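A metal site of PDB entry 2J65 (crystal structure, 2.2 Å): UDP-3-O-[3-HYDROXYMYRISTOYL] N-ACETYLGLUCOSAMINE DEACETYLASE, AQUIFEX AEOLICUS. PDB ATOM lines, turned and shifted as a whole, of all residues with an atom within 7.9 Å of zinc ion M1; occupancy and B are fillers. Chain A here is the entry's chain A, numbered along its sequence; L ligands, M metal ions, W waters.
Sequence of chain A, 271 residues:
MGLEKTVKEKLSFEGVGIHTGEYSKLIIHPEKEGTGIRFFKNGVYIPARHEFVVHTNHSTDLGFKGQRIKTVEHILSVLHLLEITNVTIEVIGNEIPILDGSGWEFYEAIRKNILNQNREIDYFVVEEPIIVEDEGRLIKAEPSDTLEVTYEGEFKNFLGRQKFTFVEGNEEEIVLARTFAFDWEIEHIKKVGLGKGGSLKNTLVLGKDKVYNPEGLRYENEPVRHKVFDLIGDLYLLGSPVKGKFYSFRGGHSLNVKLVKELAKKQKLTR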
ATOM      1  N   HIS A  58       2.157 -12.504   9.572  1.00  0.00           N
ATOM      2  CA  HIS A  58       3.346 -13.318   9.835  1.00  0.00           C
ATOM      3  C   HIS A  58       3.661 -14.305   8.685  1.00  0.00           C
ATOM      4  O   HIS A  58       4.350 -15.308   8.896  1.00  0.00           O
ATOM      5  CB  HIS A  58       3.181 -14.050  11.188  1.00  0.00           C
ATOM      6  CG  HIS A  58       3.049 -13.117  12.349  1.00  0.00           C
ATOM      7  ND1 HIS A  58       4.149 -12.592  13.000  1.00  0.00           N
ATOM      8  CD2 HIS A  58       1.961 -12.588  12.952  1.00  0.00           C
ATOM      9  CE1 HIS A  58       3.738 -11.800  13.975  1.00  0.00           C
ATOM     10  NE2 HIS A  58       2.416 -11.775  13.975  1.00  0.00           N
ATOM     11  N   SER A  59       3.146 -13.987   7.507  1.00  0.00           N
ATOM     12  CA  SER A  59       3.314 -14.743   6.252  1.00  0.00           C
ATOM     13  C   SER A  59       2.434 -14.048   5.209  1.00  0.00           C
ATOM     14  O   SER A  59       1.596 -13.204   5.563  1.00  0.00           O
ATOM     15  CB  SER A  59       2.892 -16.215   6.402  1.00  0.00           C
ATOM     16  OG  SER A  59       1.523 -16.345   6.783  1.00  0.00           O
ATOM     17  N   THR A  71       1.479 -18.997   3.563  1.00  0.00           N
ATOM     18  CA  THR A  71       2.950 -18.984   3.455  1.00  0.00           C
ATOM     19  C   THR A  71       3.466 -19.245   2.032  1.00  0.00           C
ATOM     20  O   THR A  71       4.257 -20.143   1.798  1.00  0.00           O
ATOM     21  CB  THR A  71       3.621 -19.933   4.508  1.00  0.00           C
ATOM     22  OG1 THR A  71       2.903 -19.860   5.741  1.00  0.00           O
ATOM     23  CG2 THR A  71       5.066 -19.527   4.773  1.00  0.00           C
ATOM     24  N   GLU A  73       5.235 -17.001   0.194  1.00  0.00           N
ATOM     25  CA  GLU A  73       6.341 -16.084  -0.138  1.00  0.00           C
ATOM     26  C   GLU A  73       7.625 -16.744  -0.657  1.00  0.00           C
ATOM     27  O   GLU A  73       8.284 -16.207  -1.535  1.00  0.00           O
ATOM     28  CB  GLU A  73       6.660 -15.133   1.035  1.00  0.00           C
ATOM     29  CG  GLU A  73       7.014 -15.824   2.372  1.00  0.00           C
ATOM     30  CD  GLU A  73       5.825 -15.945   3.325  1.00  0.00           C
ATOM     31  OE1 GLU A  73       4.666 -15.968   2.872  1.00  0.00           O
ATOM     32  OE2 GLU A  73       6.049 -16.027   4.545  1.00  0.00           O
ATOM     33  N   HIS A  74       7.974 -17.919  -0.124  1.00  0.00           N
ATOM     34  CA  HIS A  74       9.222 -18.576  -0.502  1.00  0.00           C
ATOM     35  C   HIS A  74       9.170 -19.317  -1.840  1.00  0.00           C
ATOM     36  O   HIS A  74      10.108 -19.191  -2.638  1.00  0.00           O
ATOM     37  CB  HIS A  74       9.731 -19.503   0.608  1.00  0.00           C
ATOM     38  CG  HIS A  74       9.911 -18.817   1.936  1.00  0.00           C
ATOM     39  ND1 HIS A  74      10.003 -19.518   3.118  1.00  0.00           N
ATOM     40  CD2 HIS A  74      10.026 -17.503   2.257  1.00  0.00           C
ATOM     41  CE1 HIS A  74      10.158 -18.663   4.117  1.00  0.00           C
ATOM     42  NE2 HIS A  74      10.164 -17.435   3.623  1.00  0.00           N
ATOM     43  N   ILE A  98       7.468 -25.564   4.861  1.00  0.00           N
ATOM     44  CA  ILE A  98       8.499 -24.580   5.177  1.00  0.00           C
ATOM     45  C   ILE A  98       9.900 -25.111   4.863  1.00  0.00           C
ATOM     46  O   ILE A  98      10.824 -24.333   4.577  1.00  0.00           O
ATOM     47  CB  ILE A  98       8.414 -24.090   6.661  1.00  0.00           C
ATOM     48  CG1 ILE A  98       9.413 -22.950   6.933  1.00  0.00           C
ATOM     49  CG2 ILE A  98       8.677 -25.249   7.633  1.00  0.00           C
ATOM     50  CD1 ILE A  98       9.073 -21.625   6.252  1.00  0.00           C
ATOM     51  N   GLY A 101      13.311 -23.532   5.950  1.00  0.00           N
ATOM     52  CA  GLY A 101      13.049 -22.094   6.149  1.00  0.00           C
ATOM     53  C   GLY A 101      13.621 -21.171   5.072  1.00  0.00           C
ATOM     54  O   GLY A 101      13.475 -19.968   5.161  1.00  0.00           O
ATOM     55  N   SER A 102      14.267 -21.749   4.065  1.00  0.00           N
ATOM     56  CA  SER A 102      14.865 -21.005   2.968  1.00  0.00           C
ATOM     57  C   SER A 102      14.265 -21.450   1.641  1.00  0.00           C
ATOM     58  O   SER A 102      13.285 -22.210   1.615  1.00  0.00           O
ATOM     59  CB  SER A 102      16.406 -21.155   2.972  1.00  0.00           C
ATOM     60  OG  SER A 102      16.829 -22.404   2.439  1.00  0.00           O
ATOM     61  N   ALA A 177      19.239 -18.263   2.621  1.00  0.00           N
ATOM     62  CA  ALA A 177      18.916 -17.500   3.832  1.00  0.00           C
ATOM     63  C   ALA A 177      17.555 -17.879   4.456  1.00  0.00           C
ATOM     64  O   ALA A 177      16.507 -17.848   3.793  1.00  0.00           O
ATOM     65  CB  ALA A 177      19.042 -15.976   3.592  1.00  0.00           C
ATOM     66  N   ARG A 178      17.593 -18.219   5.735  1.00  0.00           N
ATOM     67  CA  ARG A 178      16.410 -18.788   6.406  1.00  0.00           C
ATOM     68  C   ARG A 178      15.532 -17.783   7.119  1.00  0.00           C
ATOM     69  O   ARG A 178      15.990 -16.702   7.521  1.00  0.00           O
ATOM     70  CB  ARG A 178      16.825 -19.853   7.404  1.00  0.00           C
ATOM     71  CG  ARG A 178      17.596 -20.975   6.771  1.00  0.00           C
ATOM     72  CD  ARG A 178      17.657 -22.146   7.716  1.00  0.00           C
ATOM     73  NE  ARG A 178      18.706 -22.001   8.706  1.00  0.00           N
ATOM     74  CZ  ARG A 178      18.746 -22.675   9.847  1.00  0.00           C
ATOM     75  NH1 ARG A 178      19.760 -22.473  10.681  1.00  0.00           N
ATOM     76  NH2 ARG A 178      17.769 -23.536  10.177  1.00  0.00           N
ATOM     77  N   THR A 179      14.264 -18.160   7.240  1.00  0.00           N
ATOM     78  CA  THR A 179      13.305 -17.397   8.029  1.00  0.00           C
ATOM     79  C   THR A 179      13.797 -17.301   9.478  1.00  0.00           C
ATOM     80  O   THR A 179      14.532 -18.156   9.970  1.00  0.00           O
ATOM     81  CB  THR A 179      11.828 -17.952   7.910  1.00  0.00           C
ATOM     82  OG1 THR A 179      10.901 -16.867   8.018  1.00  0.00           O
ATOM     83  CG2 THR A 179      11.504 -18.978   8.986  1.00  0.00           C
ATOM     84  N   PHE A 180      13.434 -16.201  10.129  1.00  0.00           N
ATOM     85  CA  PHE A 180      13.952 -15.925  11.455  1.00  0.00           C
ATOM     86  C   PHE A 180      12.887 -15.355  12.377  1.00  0.00           C
ATOM     87  O   PHE A 180      11.910 -14.758  11.922  1.00  0.00           O
ATOM     88  CB  PHE A 180      15.193 -15.009  11.378  1.00  0.00           C
ATOM     89  CG  PHE A 180      14.891 -13.627  10.887  1.00  0.00           C
ATOM     90  CD1 PHE A 180      14.617 -12.600  11.795  1.00  0.00           C
ATOM     91  CD2 PHE A 180      14.845 -13.357   9.516  1.00  0.00           C
ATOM     92  CE1 PHE A 180      14.312 -11.311  11.342  1.00  0.00           C
ATOM     93  CE2 PHE A 180      14.550 -12.067   9.046  1.00  0.00           C
ATOM     94  CZ  PHE A 180      14.283 -11.044   9.959  1.00  0.00           C
ATOM     95  N   HIS A 226      17.381 -12.744   4.018  1.00  0.00           N
ATOM     96  CA  HIS A 226      16.065 -13.381   3.988  1.00  0.00           C
ATOM     97  C   HIS A 226      14.953 -12.387   3.701  1.00  0.00           C
ATOM     98  O   HIS A 226      13.983 -12.711   3.025  1.00  0.00           O
ATOM     99  CB  HIS A 226      15.717 -14.154   5.266  1.00  0.00           C
ATOM    100  CG  HIS A 226      14.476 -14.966   5.105  1.00  0.00           C
ATOM    101  ND1 HIS A 226      14.480 -16.195   4.477  1.00  0.00           N
ATOM    102  CD2 HIS A 226      13.188 -14.693   5.410  1.00  0.00           C
ATOM    103  CE1 HIS A 226      13.251 -16.663   4.440  1.00  0.00           C
ATOM    104  NE2 HIS A 226      12.449 -15.777   4.993  1.00  0.00           N
ATOM    105  N   LYS A 227      15.076 -11.190   4.251  1.00  0.00           N
ATOM    106  CA  LYS A 227      14.111 -10.133   3.986  1.00  0.00           C
ATOM    107  C   LYS A 227      14.100  -9.707   2.520  1.00  0.00           C
ATOM    108  O   LYS A 227      13.036  -9.406   1.969  1.00  0.00           O
ATOM    109  CB  LYS A 227      14.337  -8.949   4.910  1.00  0.00           C
ATOM    110  CG  LYS A 227      13.886  -9.190   6.361  1.00  0.00           C
ATOM    111  CD  LYS A 227      12.372  -9.126   6.471  1.00  0.00           C
ATOM    112  CE  LYS A 227      11.910  -9.026   7.916  1.00  0.00           C
ATOM    113  NZ  LYS A 227      10.501  -8.540   8.000  1.00  0.00           N
ATOM    114  N   PHE A 229      14.895 -11.786   0.032  1.00  0.00           N
ATOM    115  CA  PHE A 229      14.254 -12.973  -0.521  1.00  0.00           C
ATOM    116  C   PHE A 229      12.712 -12.937  -0.394  1.00  0.00           C
ATOM    117  O   PHE A 229      12.018 -13.265  -1.362  1.00  0.00           O
ATOM    118  CB  PHE A 229      14.828 -14.208   0.152  1.00  0.00           C
ATOM    119  CG  PHE A 229      14.222 -15.517  -0.295  1.00  0.00           C
ATOM    120  CD1 PHE A 229      14.496 -16.041  -1.565  1.00  0.00           C
ATOM    121  CD2 PHE A 229      13.407 -16.243   0.570  1.00  0.00           C
ATOM    122  CE1 PHE A 229      13.955 -17.260  -1.956  1.00  0.00           C
ATOM    123  CE2 PHE A 229      12.843 -17.463   0.177  1.00  0.00           C
ATOM    124  CZ  PHE A 229      13.116 -17.978  -1.081  1.00  0.00           C
ATOM    125  N   ASP A 230      12.203 -12.536   0.775  1.00  0.00           N
ATOM    126  CA  ASP A 230      10.761 -12.339   1.007  1.00  0.00           C
ATOM    127  C   ASP A 230      10.175 -11.263   0.071  1.00  0.00           C
ATOM    128  O   ASP A 230       9.120 -11.475  -0.508  1.00  0.00           O
ATOM    129  CB  ASP A 230      10.468 -11.914   2.457  1.00  0.00           C
ATOM    130  CG  ASP A 230      10.454 -13.079   3.451  1.00  0.00           C
ATOM    131  OD1 ASP A 230      10.324 -14.250   3.039  1.00  0.00           O
ATOM    132  OD2 ASP A 230      10.549 -12.800   4.666  1.00  0.00           O
ATOM    133  N   LEU A 231      10.845 -10.120  -0.060  1.00  0.00           N
ATOM    134  CA  LEU A 231      10.332  -9.039  -0.906  1.00  0.00           C
ATOM    135  C   LEU A 231      10.201  -9.453  -2.385  1.00  0.00           C
ATOM    136  O   LEU A 231       9.221  -9.104  -3.056  1.00  0.00           O
ATOM    137  CB  LEU A 231      11.208  -7.788  -0.757  1.00  0.00           C
ATOM    138  CG  LEU A 231      10.955  -6.484  -1.527  1.00  0.00           C
ATOM    139  CD1 LEU A 231       9.484  -6.021  -1.597  1.00  0.00           C
ATOM    140  CD2 LEU A 231      11.816  -5.387  -0.909  1.00  0.00           C
ATOM    141  N   HIS A 253       6.035  -8.237   5.103  1.00  0.00           N
ATOM    142  CA  HIS A 253       4.973  -8.637   4.169  1.00  0.00           C
ATOM    143  C   HIS A 253       3.846  -7.601   3.982  1.00  0.00           C
ATOM    144  O   HIS A 253       3.419  -7.343   2.863  1.00  0.00           O
ATOM    145  CB  HIS A 253       4.387  -9.999   4.557  1.00  0.00           C
ATOM    146  CG  HIS A 253       5.400 -11.107   4.602  1.00  0.00           C
ATOM    147  ND1 HIS A 253       6.096 -11.520   3.485  1.00  0.00           N
ATOM    148  CD2 HIS A 253       5.812 -11.899   5.618  1.00  0.00           C
ATOM    149  CE1 HIS A 253       6.907 -12.509   3.826  1.00  0.00           C
ATOM    150  NE2 HIS A 253       6.745 -12.769   5.109  1.00  0.00           N
HETATM  151  C1  LIG L   1       7.436 -14.053   8.536  1.00  0.00           C
HETATM  152  O1  LIG L   1       6.752 -14.771   7.780  1.00  0.00           O
HETATM  153  O2  LIG L   1       7.454 -12.807   8.376  1.00  0.00           O
HETATM  154  C2  LIG L   1       8.249 -14.703   9.635  1.00  0.00           C
HETATM  155  C3  LIG L   1       7.353 -15.071  10.814  1.00  0.00           C
HETATM  156  C4  LIG L   1       8.182 -15.730  11.922  1.00  0.00           C
HETATM  157  C5  LIG L   1       8.132 -17.251  11.812  1.00  0.00           C
HETATM  158  C6  LIG L   1       7.466 -17.847  13.042  1.00  0.00           C
HETATM  159  C7  LIG L   1       8.318 -18.967  13.608  1.00  0.00           C
HETATM  160  C8  LIG L   1       7.626 -19.648  14.782  1.00  0.00           C
HETATM  161  C9  LIG L   1       8.332 -19.316  16.095  1.00  0.00           C
HETATM  162  C10 LIG L   1       8.348 -20.540  16.986  1.00  0.00           C
HETATM  163  C11 LIG L   1       9.665 -21.282  16.864  1.00  0.00           C
HETATM  164  C12 LIG L   1      10.219 -21.572  18.242  1.00  0.00           C
HETATM  165  C13 LIG L   1      10.714 -23.005  18.320  1.00  0.00           C
HETATM  166  C14 LIG L   1      12.221 -23.030  18.510  1.00  0.00           C
HETATM  167 ZN    ZN M   1      10.449 -15.578   4.592  1.00  0.00          ZN
HETATM  168 ZN    ZN M   2       7.436 -14.623   5.647  1.00  0.00          ZN
HETATM  169  O   HOH W   1       9.228 -15.580   6.151  1.00  0.00           O
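The backbone NH of Thr 179 sits at hydrogen-bond distance from the backbone carbonyl oxygen of Gly 101, at 2.9 Å. O of Ala 177 lies within hydrogen-bond range of ND1 of His 226 (2.7 Å). ND1 of His 226 sits close to N of Thr 179. ND1 of His 226 sits close to O of Arg 178, at 3.4 Å.
Thr 179 touches zinc ion M1 (OG1 to ZN, 3.7 Å).
An oxygen (O1) of the ligand lies close to the backbone carbonyl oxygen of His 58, at 2.7 Å.
Water W1 bridges OG1 of Thr 179 (2.8 Å) and OD2 of Asp 230 (3.4 Å).
Zinc ion M1 is bound by water W1, OD1 of Asp 230, NE2 of His 226 and NE2 of His 74. Zinc ion M1 has four donor atoms within binding distance. Slightly farther from zinc ion M1 lies OD2 of Asp 230 (2.8 Å).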
